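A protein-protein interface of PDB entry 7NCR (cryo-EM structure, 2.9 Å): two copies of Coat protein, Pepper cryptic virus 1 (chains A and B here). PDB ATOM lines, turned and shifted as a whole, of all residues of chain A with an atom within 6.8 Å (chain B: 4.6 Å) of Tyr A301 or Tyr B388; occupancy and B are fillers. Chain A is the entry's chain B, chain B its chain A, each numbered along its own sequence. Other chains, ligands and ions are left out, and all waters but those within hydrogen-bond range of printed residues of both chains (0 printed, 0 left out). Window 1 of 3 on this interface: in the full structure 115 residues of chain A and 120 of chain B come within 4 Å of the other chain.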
ATOM      1  N   CYS A 240      27.435  -3.631  -1.253  1.00  0.00           N
ATOM      2  CA  CYS A 240      26.214  -2.850  -1.354  1.00  0.00           C
ATOM      3  C   CYS A 240      25.048  -3.569  -0.699  1.00  0.00           C
ATOM      4  O   CYS A 240      24.873  -4.776  -0.870  1.00  0.00           O
ATOM      5  CB  CYS A 240      25.893  -2.552  -2.815  1.00  0.00           C
ATOM      6  SG  CYS A 240      27.124  -1.563  -3.658  1.00  0.00           S
ATOM      7  N   ALA A 241      24.243  -2.806   0.033  1.00  0.00           N
ATOM      8  CA  ALA A 241      23.127  -3.336   0.805  1.00  0.00           C
ATOM      9  C   ALA A 241      21.875  -3.375  -0.060  1.00  0.00           C
ATOM     10  O   ALA A 241      21.407  -2.332  -0.524  1.00  0.00           O
ATOM     11  CB  ALA A 241      22.888  -2.482   2.044  1.00  0.00           C
ATOM     12  N   TRP A 242      21.341  -4.569  -0.281  1.00  0.00           N
ATOM     13  CA  TRP A 242      20.117  -4.729  -1.048  1.00  0.00           C
ATOM     14  C   TRP A 242      18.874  -4.584  -0.192  1.00  0.00           C
ATOM     15  O   TRP A 242      17.789  -4.972  -0.626  1.00  0.00           O
ATOM     16  CB  TRP A 242      20.100  -6.085  -1.758  1.00  0.00           C
ATOM     17  CG  TRP A 242      20.494  -7.237  -0.901  1.00  0.00           C
ATOM     18  CD1 TRP A 242      21.739  -7.738  -0.737  1.00  0.00           C
ATOM     19  CD2 TRP A 242      19.626  -8.044  -0.096  1.00  0.00           C
ATOM     20  NE1 TRP A 242      21.714  -8.803   0.125  1.00  0.00           N
ATOM     21  CE2 TRP A 242      20.426  -9.009   0.536  1.00  0.00           C
ATOM     22  CE3 TRP A 242      18.252  -8.036   0.161  1.00  0.00           C
ATOM     23  CZ2 TRP A 242      19.899  -9.962   1.402  1.00  0.00           C
ATOM     24  CZ3 TRP A 242      17.735  -8.976   1.023  1.00  0.00           C
ATOM     25  CH2 TRP A 242      18.555  -9.925   1.633  1.00  0.00           C
ATOM     26  N   GLY A 269      20.845  -9.678  -4.227  1.00  0.00           N
ATOM     27  CA  GLY A 269      20.167  -8.434  -4.488  1.00  0.00           C
ATOM     28  C   GLY A 269      19.496  -8.382  -5.841  1.00  0.00           C
ATOM     29  O   GLY A 269      19.723  -9.228  -6.705  1.00  0.00           O
ATOM     30  N   PRO A 270      18.664  -7.369  -6.051  1.00  0.00           N
ATOM     31  CA  PRO A 270      17.924  -7.270  -7.309  1.00  0.00           C
ATOM     32  C   PRO A 270      18.838  -6.940  -8.476  1.00  0.00           C
ATOM     33  O   PRO A 270      19.916  -6.366  -8.321  1.00  0.00           O
ATOM     34  CB  PRO A 270      16.931  -6.132  -7.055  1.00  0.00           C
ATOM     35  CG  PRO A 270      17.026  -5.826  -5.618  1.00  0.00           C
ATOM     36  CD  PRO A 270      18.369  -6.241  -5.163  1.00  0.00           C
ATOM     37  N   SER A 271      18.375  -7.307  -9.664  1.00  0.00           N
ATOM     38  CA  SER A 271      19.128  -7.083 -10.887  1.00  0.00           C
ATOM     39  C   SER A 271      18.152  -6.832 -12.025  1.00  0.00           C
ATOM     40  O   SER A 271      17.148  -7.531 -12.154  1.00  0.00           O
ATOM     41  CB  SER A 271      20.027  -8.278 -11.208  1.00  0.00           C
ATOM     42  OG  SER A 271      20.837  -8.018 -12.334  1.00  0.00           O
ATOM     43  N   ASP A 272      18.451  -5.829 -12.842  1.00  0.00           N
ATOM     44  CA  ASP A 272      17.645  -5.483 -14.009  1.00  0.00           C
ATOM     45  C   ASP A 272      18.497  -5.752 -15.247  1.00  0.00           C
ATOM     46  O   ASP A 272      19.260  -4.897 -15.690  1.00  0.00           O
ATOM     47  CB  ASP A 272      17.190  -4.032 -13.944  1.00  0.00           C
ATOM     48  CG  ASP A 272      16.192  -3.684 -15.025  1.00  0.00           C
ATOM     49  OD1 ASP A 272      15.334  -4.529 -15.342  1.00  0.00           O
ATOM     50  OD2 ASP A 272      16.264  -2.564 -15.562  1.00  0.00           O
ATOM     51  N   ASP A 273      18.364  -6.951 -15.802  1.00  0.00           N
ATOM     52  CA  ASP A 273      19.185  -7.362 -16.930  1.00  0.00           C
ATOM     53  C   ASP A 273      18.452  -7.153 -18.246  1.00  0.00           C
ATOM     54  O   ASP A 273      17.222  -7.140 -18.301  1.00  0.00           O
ATOM     55  CB  ASP A 273      19.594  -8.825 -16.791  1.00  0.00           C
ATOM     56  CG  ASP A 273      18.518  -9.668 -16.165  1.00  0.00           C
ATOM     57  OD1 ASP A 273      17.402  -9.146 -15.968  1.00  0.00           O
ATOM     58  OD2 ASP A 273      18.787 -10.850 -15.867  1.00  0.00           O
ATOM     59  N   ASN A 297      15.453  -0.981 -22.514  1.00  0.00           N
ATOM     60  CA  ASN A 297      15.428   0.129 -21.576  1.00  0.00           C
ATOM     61  C   ASN A 297      15.215  -0.375 -20.156  1.00  0.00           C
ATOM     62  O   ASN A 297      14.582  -1.407 -19.924  1.00  0.00           O
ATOM     63  CB  ASN A 297      14.332   1.128 -21.942  1.00  0.00           C
ATOM     64  CG  ASN A 297      14.205   1.330 -23.434  1.00  0.00           C
ATOM     65  OD1 ASN A 297      15.046   1.977 -24.058  1.00  0.00           O
ATOM     66  ND2 ASN A 297      13.150   0.774 -24.018  1.00  0.00           N
ATOM     67  N   ARG A 298      15.746   0.378 -19.201  1.00  0.00           N
ATOM     68  CA  ARG A 298      15.715  -0.031 -17.808  1.00  0.00           C
ATOM     69  C   ARG A 298      14.306   0.058 -17.236  1.00  0.00           C
ATOM     70  O   ARG A 298      13.507   0.917 -17.614  1.00  0.00           O
ATOM     71  CB  ARG A 298      16.665   0.835 -16.987  1.00  0.00           C
ATOM     72  CG  ARG A 298      18.080   0.861 -17.508  1.00  0.00           C
ATOM     73  CD  ARG A 298      18.931  -0.171 -16.807  1.00  0.00           C
ATOM     74  NE  ARG A 298      19.391   0.289 -15.503  1.00  0.00           N
ATOM     75  CZ  ARG A 298      18.814  -0.038 -14.357  1.00  0.00           C
ATOM     76  NH1 ARG A 298      17.757  -0.828 -14.358  1.00  0.00           N
ATOM     77  NH2 ARG A 298      19.290   0.422 -13.212  1.00  0.00           N
ATOM     78  N   ARG A 299      14.010  -0.840 -16.302  1.00  0.00           N
ATOM     79  CA  ARG A 299      12.709  -0.918 -15.654  1.00  0.00           C
ATOM     80  C   ARG A 299      12.752  -0.514 -14.190  1.00  0.00           C
ATOM     81  O   ARG A 299      11.924   0.285 -13.744  1.00  0.00           O
ATOM     82  CB  ARG A 299      12.151  -2.342 -15.776  1.00  0.00           C
ATOM     83  CG  ARG A 299      11.492  -2.649 -17.104  1.00  0.00           C
ATOM     84  CD  ARG A 299      10.140  -3.316 -16.905  1.00  0.00           C
ATOM     85  NE  ARG A 299       9.210  -2.465 -16.168  1.00  0.00           N
ATOM     86  CZ  ARG A 299       8.956  -2.577 -14.866  1.00  0.00           C
ATOM     87  NH1 ARG A 299       9.557  -3.511 -14.147  1.00  0.00           N
ATOM     88  NH2 ARG A 299       8.098  -1.752 -14.288  1.00  0.00           N
ATOM     89  N   SER A 300      13.702  -1.047 -13.427  1.00  0.00           N
ATOM     90  CA  SER A 300      13.791  -0.805 -11.997  1.00  0.00           C
ATOM     91  C   SER A 300      15.130  -0.168 -11.667  1.00  0.00           C
ATOM     92  O   SER A 300      16.129  -0.399 -12.352  1.00  0.00           O
ATOM     93  CB  SER A 300      13.613  -2.100 -11.211  1.00  0.00           C
ATOM     94  OG  SER A 300      12.433  -2.772 -11.607  1.00  0.00           O
ATOM     95  N   TYR A 301      15.147   0.631 -10.605  1.00  0.00           N
ATOM     96  CA  TYR A 301      16.306   1.448 -10.288  1.00  0.00           C
ATOM     97  C   TYR A 301      16.586   1.404  -8.794  1.00  0.00           C
ATOM     98  O   TYR A 301      15.727   1.053  -7.987  1.00  0.00           O
ATOM     99  CB  TYR A 301      16.101   2.898 -10.735  1.00  0.00           C
ATOM    100  CG  TYR A 301      15.665   3.035 -12.168  1.00  0.00           C
ATOM    101  CD1 TYR A 301      14.322   3.122 -12.497  1.00  0.00           C
ATOM    102  CD2 TYR A 301      16.593   3.064 -13.193  1.00  0.00           C
ATOM    103  CE1 TYR A 301      13.919   3.238 -13.806  1.00  0.00           C
ATOM    104  CE2 TYR A 301      16.202   3.184 -14.495  1.00  0.00           C
ATOM    105  CZ  TYR A 301      14.865   3.268 -14.801  1.00  0.00           C
ATOM    106  OH  TYR A 301      14.473   3.387 -16.111  1.00  0.00           O
ATOM    107  N   GLY A 302      17.818   1.770  -8.446  1.00  0.00           N
ATOM    108  CA  GLY A 302      18.215   1.891  -7.061  1.00  0.00           C
ATOM    109  C   GLY A 302      19.075   3.123  -6.877  1.00  0.00           C
ATOM    110  O   GLY A 302      19.447   3.792  -7.839  1.00  0.00           O
ATOM    111  N   ALA A 303      19.381   3.417  -5.615  1.00  0.00           N
ATOM    112  CA  ALA A 303      20.248   4.550  -5.323  1.00  0.00           C
ATOM    113  C   ALA A 303      21.676   4.280  -5.774  1.00  0.00           C
ATOM    114  O   ALA A 303      22.337   5.166  -6.322  1.00  0.00           O
ATOM    115  CB  ALA A 303      20.205   4.876  -3.835  1.00  0.00           C
ATOM    116  N   TYR A 304      22.169   3.070  -5.551  1.00  0.00           N
ATOM    117  CA  TYR A 304      23.480   2.654  -6.017  1.00  0.00           C
ATOM    118  C   TYR A 304      23.308   1.480  -6.964  1.00  0.00           C
ATOM    119  O   TYR A 304      22.507   0.583  -6.702  1.00  0.00           O
ATOM    120  CB  TYR A 304      24.389   2.269  -4.850  1.00  0.00           C
ATOM    121  CG  TYR A 304      25.843   2.230  -5.227  1.00  0.00           C
ATOM    122  CD1 TYR A 304      26.379   1.129  -5.871  1.00  0.00           C
ATOM    123  CD2 TYR A 304      26.678   3.299  -4.947  1.00  0.00           C
ATOM    124  CE1 TYR A 304      27.702   1.090  -6.223  1.00  0.00           C
ATOM    125  CE2 TYR A 304      28.002   3.267  -5.294  1.00  0.00           C
ATOM    126  CZ  TYR A 304      28.509   2.158  -5.934  1.00  0.00           C
ATOM    127  OH  TYR A 304      29.833   2.111  -6.288  1.00  0.00           O
ATOM    128  N   GLU A 305      24.047   1.493  -8.066  1.00  0.00           N
ATOM    129  CA  GLU A 305      23.936   0.450  -9.071  1.00  0.00           C
ATOM    130  C   GLU A 305      25.310  -0.005  -9.532  1.00  0.00           C
ATOM    131  O   GLU A 305      26.239   0.796  -9.642  1.00  0.00           O
ATOM    132  CB  GLU A 305      23.122   0.927 -10.268  1.00  0.00           C
ATOM    133  CG  GLU A 305      21.753   1.451  -9.907  1.00  0.00           C
ATOM    134  CD  GLU A 305      20.973   1.903 -11.109  1.00  0.00           C
ATOM    135  OE1 GLU A 305      21.597   2.166 -12.155  1.00  0.00           O
ATOM    136  OE2 GLU A 305      19.733   1.977 -11.017  1.00  0.00           O
ATOM    137  N   VAL A 306      25.420  -1.297  -9.815  1.00  0.00           N
ATOM    138  CA  VAL A 306      26.630  -1.908 -10.350  1.00  0.00           C
ATOM    139  C   VAL A 306      26.256  -2.594 -11.653  1.00  0.00           C
ATOM    140  O   VAL A 306      25.286  -3.353 -11.696  1.00  0.00           O
ATOM    141  CB  VAL A 306      27.244  -2.921  -9.364  1.00  0.00           C
ATOM    142  CG1 VAL A 306      28.496  -3.540  -9.943  1.00  0.00           C
ATOM    143  CG2 VAL A 306      27.536  -2.263  -8.035  1.00  0.00           C
ATOM    144  N   TYR A 388       6.738  -9.197  -8.442  1.00  0.00           N
ATOM    145  CA  TYR A 388       6.690  -9.376  -7.002  1.00  0.00           C
ATOM    146  C   TYR A 388       6.466  -8.029  -6.342  1.00  0.00           C
ATOM    147  O   TYR A 388       6.969  -7.008  -6.817  1.00  0.00           O
ATOM    148  CB  TYR A 388       7.958 -10.047  -6.473  1.00  0.00           C
ATOM    149  CG  TYR A 388       9.252  -9.388  -6.858  1.00  0.00           C
ATOM    150  CD1 TYR A 388       9.827  -9.613  -8.096  1.00  0.00           C
ATOM    151  CD2 TYR A 388       9.913  -8.560  -5.969  1.00  0.00           C
ATOM    152  CE1 TYR A 388      11.014  -9.016  -8.440  1.00  0.00           C
ATOM    153  CE2 TYR A 388      11.095  -7.966  -6.303  1.00  0.00           C
ATOM    154  CZ  TYR A 388      11.642  -8.195  -7.538  1.00  0.00           C
ATOM    155  OH  TYR A 388      12.826  -7.596  -7.867  1.00  0.00           O
ATOM    156  N   ARG B  48      22.599   8.308  -6.366  1.00  0.00           N
ATOM    157  CA  ARG B  48      21.408   9.081  -6.669  1.00  0.00           C
ATOM    158  C   ARG B  48      20.957   9.836  -5.431  1.00  0.00           C
ATOM    159  O   ARG B  48      20.975   9.293  -4.324  1.00  0.00           O
ATOM    160  CB  ARG B  48      20.287   8.174  -7.170  1.00  0.00           C
ATOM    161  CG  ARG B  48      20.595   7.528  -8.488  1.00  0.00           C
ATOM    162  CD  ARG B  48      19.344   7.221  -9.263  1.00  0.00           C
ATOM    163  NE  ARG B  48      19.646   6.895 -10.651  1.00  0.00           N
ATOM    164  CZ  ARG B  48      19.560   5.675 -11.166  1.00  0.00           C
ATOM    165  NH1 ARG B  48      19.174   4.665 -10.405  1.00  0.00           N
ATOM    166  NH2 ARG B  48      19.855   5.464 -12.438  1.00  0.00           N
ATOM    167  N   ARG B  54      11.294  11.324 -11.034  1.00  0.00           N
ATOM    168  CA  ARG B  54      10.875  10.365 -12.051  1.00  0.00           C
ATOM    169  C   ARG B  54       9.524  10.790 -12.590  1.00  0.00           C
ATOM    170  O   ARG B  54       8.555  10.851 -11.834  1.00  0.00           O
ATOM    171  CB  ARG B  54      10.782   8.948 -11.487  1.00  0.00           C
ATOM    172  CG  ARG B  54      12.103   8.304 -11.235  1.00  0.00           C
ATOM    173  CD  ARG B  54      12.179   6.932 -11.840  1.00  0.00           C
ATOM    174  NE  ARG B  54      13.566   6.496 -11.888  1.00  0.00           N
ATOM    175  CZ  ARG B  54      14.352   6.647 -12.943  1.00  0.00           C
ATOM    176  NH1 ARG B  54      13.879   7.204 -14.046  1.00  0.00           N
ATOM    177  NH2 ARG B  54      15.610   6.234 -12.896  1.00  0.00           N
ATOM    178  N   PRO B 164      14.510   0.552  -3.245  1.00  0.00           N
ATOM    179  CA  PRO B 164      15.947   0.697  -3.543  1.00  0.00           C
ATOM    180  C   PRO B 164      16.351   2.108  -3.933  1.00  0.00           C
ATOM    181  O   PRO B 164      17.432   2.568  -3.552  1.00  0.00           O
ATOM    182  CB  PRO B 164      16.158  -0.293  -4.693  1.00  0.00           C
ATOM    183  CG  PRO B 164      15.155  -1.322  -4.468  1.00  0.00           C
ATOM    184  CD  PRO B 164      13.957  -0.667  -3.856  1.00  0.00           C
ATOM    185  N   GLU B 165      15.503   2.815  -4.665  1.00  0.00           N
ATOM    186  CA  GLU B 165      15.751   4.193  -5.057  1.00  0.00           C
ATOM    187  C   GLU B 165      14.756   5.079  -4.327  1.00  0.00           C
ATOM    188  O   GLU B 165      13.548   4.976  -4.553  1.00  0.00           O
ATOM    189  CB  GLU B 165      15.631   4.355  -6.566  1.00  0.00           C
ATOM    190  CG  GLU B 165      15.626   5.784  -7.034  1.00  0.00           C
ATOM    191  CD  GLU B 165      15.634   5.895  -8.537  1.00  0.00           C
ATOM    192  OE1 GLU B 165      16.668   5.576  -9.146  1.00  0.00           O
ATOM    193  OE2 GLU B 165      14.601   6.287  -9.115  1.00  0.00           O
ATOM    194  N   PRO B 270       8.615  -4.190  -9.745  1.00  0.00           N
ATOM    195  CA  PRO B 270       9.650  -5.082 -10.263  1.00  0.00           C
ATOM    196  C   PRO B 270       9.067  -6.422 -10.680  1.00  0.00           C
ATOM    197  O   PRO B 270       8.018  -6.857 -10.206  1.00  0.00           O
ATOM    198  CB  PRO B 270      10.605  -5.251  -9.077  1.00  0.00           C
ATOM    199  CG  PRO B 270       9.919  -4.638  -7.897  1.00  0.00           C
ATOM    200  CD  PRO B 270       8.542  -4.236  -8.281  1.00  0.00           C
ATOM    201  N   ASP B 386      22.289  -5.173 -14.554  1.00  0.00           N
ATOM    202  CA  ASP B 386      22.351  -3.931 -13.795  1.00  0.00           C
ATOM    203  C   ASP B 386      21.785  -4.188 -12.408  1.00  0.00           C
ATOM    204  O   ASP B 386      20.566  -4.205 -12.219  1.00  0.00           O
ATOM    205  CB  ASP B 386      21.592  -2.815 -14.505  1.00  0.00           C
ATOM    206  CG  ASP B 386      22.481  -2.001 -15.422  1.00  0.00           C
ATOM    207  OD1 ASP B 386      23.576  -1.597 -14.989  1.00  0.00           O
ATOM    208  OD2 ASP B 386      22.085  -1.759 -16.580  1.00  0.00           O
ATOM    209  N   TRP B 387      22.673  -4.392 -11.446  1.00  0.00           N
ATOM    210  CA  TRP B 387      22.297  -4.591 -10.059  1.00  0.00           C
ATOM    211  C   TRP B 387      22.007  -3.232  -9.448  1.00  0.00           C
ATOM    212  O   TRP B 387      22.765  -2.287  -9.662  1.00  0.00           O
ATOM    213  CB  TRP B 387      23.415  -5.290  -9.296  1.00  0.00           C
ATOM    214  CG  TRP B 387      23.942  -6.494  -9.980  1.00  0.00           C
ATOM    215  CD1 TRP B 387      24.787  -6.527 -11.043  1.00  0.00           C
ATOM    216  CD2 TRP B 387      23.674  -7.855  -9.638  1.00  0.00           C
ATOM    217  NE1 TRP B 387      25.054  -7.822 -11.393  1.00  0.00           N
ATOM    218  CE2 TRP B 387      24.383  -8.658 -10.543  1.00  0.00           C
ATOM    219  CE3 TRP B 387      22.898  -8.473  -8.651  1.00  0.00           C
ATOM    220  CZ2 TRP B 387      24.343 -10.041 -10.495  1.00  0.00           C
ATOM    221  CZ3 TRP B 387      22.858  -9.840  -8.608  1.00  0.00           C
ATOM    222  CH2 TRP B 387      23.574 -10.612  -9.523  1.00  0.00           C
ATOM    223  N   TYR B 388      20.908  -3.119  -8.719  1.00  0.00           N
ATOM    224  CA  TYR B 388      20.572  -1.877  -8.047  1.00  0.00           C
ATOM    225  C   TYR B 388      20.373  -2.145  -6.566  1.00  0.00           C
ATOM    226  O   TYR B 388      19.829  -3.182  -6.179  1.00  0.00           O
ATOM    227  CB  TYR B 388      19.331  -1.221  -8.651  1.00  0.00           C
ATOM    228  CG  TYR B 388      18.124  -2.109  -8.806  1.00  0.00           C
ATOM    229  CD1 TYR B 388      17.976  -2.925  -9.913  1.00  0.00           C
ATOM    230  CD2 TYR B 388      17.117  -2.105  -7.860  1.00  0.00           C
ATOM    231  CE1 TYR B 388      16.870  -3.723 -10.060  1.00  0.00           C
ATOM    232  CE2 TYR B 388      16.009  -2.899  -8.001  1.00  0.00           C
ATOM    233  CZ  TYR B 388      15.888  -3.703  -9.104  1.00  0.00           C
ATOM    234  OH  TYR B 388      14.780  -4.498  -9.232  1.00  0.00           O
ATOM    235  N   TYR B 389      20.834  -1.210  -5.746  1.00  0.00           N
ATOM    236  CA  TYR B 389      20.921  -1.406  -4.312  1.00  0.00           C
ATOM    237  C   TYR B 389      20.403  -0.161  -3.617  1.00  0.00           C
ATOM    238  O   TYR B 389      20.074   0.841  -4.253  1.00  0.00           O
ATOM    239  CB  TYR B 389      22.360  -1.713  -3.895  1.00  0.00           C
ATOM    240  CG  TYR B 389      22.887  -3.012  -4.447  1.00  0.00           C
ATOM    241  CD1 TYR B 389      22.485  -4.228  -3.914  1.00  0.00           C
ATOM    242  CD2 TYR B 389      23.786  -3.026  -5.493  1.00  0.00           C
ATOM    243  CE1 TYR B 389      22.957  -5.405  -4.408  1.00  0.00           C
ATOM    244  CE2 TYR B 389      24.263  -4.205  -5.990  1.00  0.00           C
ATOM    245  CZ  TYR B 389      23.842  -5.389  -5.446  1.00  0.00           C
ATOM    246  OH  TYR B 389      24.318  -6.574  -5.940  1.00  0.00           O
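The guanidinium group (NH1) of Arg B48 is in hydrogen-bond range of the backbone carbonyl oxygen (O) of Gly A302 (2.7 Å). The backbone carbonyl oxygen of Ala A303 sits at hydrogen-bond distance from the backbone NH of Arg B48, at 3.2 Å. The side-chain carboxylate (OE2) of Glu A305 lies within salt-bridge range of the guanidinium group (NH1) of Arg B48, 2.8 Å away. The backbone carbonyl oxygen of Pro B164 is in hydrogen-bond range of the backbone NH of Ala A303, 3.0 Å away. The backbone carbonyl oxygen of Pro B270 sits at hydrogen-bond distance from the backbone NH of Tyr A388 (3.2 Å). The backbone NH of Asp A272 sits at hydrogen-bond distance from the backbone carbonyl oxygen of Asp B386 (2.7 Å). The side-chain carboxylate (OD2) of Asp B386 is in salt-bridge range of the guanidinium group (NE) of Arg A298 (3.6 Å). O of Val A306 lies within hydrogen-bond range of N of Trp B387 (2.8 Å). The backbone NH of Tyr B388 sits at hydrogen-bond distance from the backbone carbonyl oxygen of Pro A270, at 3.4 Å. O of Tyr B389 is in hydrogen-bond range of N of Ala A303, at 3.0 Å. N of Tyr B389 lies within hydrogen-bond range of O of Tyr A304 (2.6 Å).
NH1 of Arg B48 lies within salt-bridge range of OE1 of Glu B165 (2.9 Å). The side-chain carboxylate of Glu B165 lies within salt-bridge range of the guanidinium group of Arg B54, 3.0 Å away. The side-chain carboxylate (OD2) of Asp A272 lies within hydrogen-bond range of the backbone NH (N) of Arg A299, at 2.9 Å. OH of Tyr A301 is in hydrogen-bond range of O of Arg A298, at 3.0 Å. OE2 of Glu A305 lies within salt-bridge range of NH2 of Arg A298, at 2.7 Å. The backbone NH (N) of Gly A302 is in hydrogen-bond range of the side-chain carboxylate (OE2) of Glu A305 (3.2 Å).
Among the printed residues, merely in contact across the chains: Cys A240 with Tyr B389 (3.4 Å), Ala A241 with Tyr B389 (3.6 Å), Trp A242 with Tyr B389 (3.7 Å), Gly A269 with Trp B387 (3.7 Å), Pro A270 with Trp B387 (3.4 Å), Ser A271 with Asp B386 (3.5 Å), Ser A271 with Trp B387 (3.8 Å), Ser A271 with Tyr B388 (3.9 Å), Asp A272 with Tyr B388 (3.8 Å), Ser A300 with Pro B270 (3.9 Å), Ser A300 with Tyr B388 (3.3 Å), Tyr A301 with Arg B48 (3.6 Å), Tyr A301 with Arg B54 (3.3 Å), Tyr A301 with Pro B164 (3.6 Å), Tyr A301 with Glu B165 (3.2 Å), Tyr A301 with Tyr B388 (3.5 Å), Gly A302 with Pro B164 (3.6 Å), Gly A302 with Glu B165 (3.6 Å), Gly A302 with Tyr B388 (3.4 Å), Gly A302 with Tyr B389 (3.5 Å), Ala A303 with Glu B165 (3.8 Å), Tyr A304 with Tyr B388 (3.4 Å), Glu A305 with Trp B387 (3.0 Å), Glu A305 with Tyr B388 (3.8 Å), Val A306 with Asp B386 (3.7 Å) and Tyr A388 with Tyr B388 (3.9 Å).
Of chain B, only Arg B48, Arg B54, Pro B164, Glu B165 and Tyr B388 come within 4 Å of Tyr A301. Tyr B388 touches just these residues of chain A: Pro A270 (3.3 Å), Ser A271 (3.9 Å), Asp A272 (3.8 Å), Ser A300 (3.3 Å), Tyr A301 (3.5 Å), Gly A302 (3.4 Å), Tyr A304 (3.4 Å), Glu A305 (3.8 Å) and Tyr A388 (3.9 Å). Printed residues of chain A within 4 Å of Glu B165: Tyr A301, Gly A302 and Ala A303. Printed residues of chain B within 4 Å of Ala A303: Arg B48, Pro B164, Glu B165 and Tyr B389. Of the printed residues of chain B, Arg A298 touches Asp B386. Arg A299 touches none of the printed residues of chain B.
Of the 9 printed residues of chain B, 9 touch a printed residue of chain A. Printed residues of chain B that touch a printed residue of chain A: Arg B48, Arg B54, Pro B164, Glu B165, Pro B270, Asp B386, Trp B387, Tyr B388 and Tyr B389. Hydrophobic or aromatic side chains of chain B that line the printed part of chain A: Pro B164, Pro B270, Trp B387, Tyr B388 and Tyr B389. Hydrophobic or aromatic side chains of chain A that line the printed part of chain B: Trp A242, Pro A270, Tyr A301, Ala A303 and Tyr A388. Among the printed residues, Asp or Glu carboxylates within 4 Å of a Lys or Arg side-chain nitrogen of the other chain: Arg A298 with Asp B386 (3.6 Å) and Glu A305 with Arg B48 (2.8 Å).
Pro A270 touches Tyr B388, and with the chains exchanged Tyr A388 touches Pro B270. Tyr B388 touches its own counterpart, Tyr A388. Of the 37 pairs that touch across the chains among the printed residues, 3 have their exchanged pair printed and touching as well.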
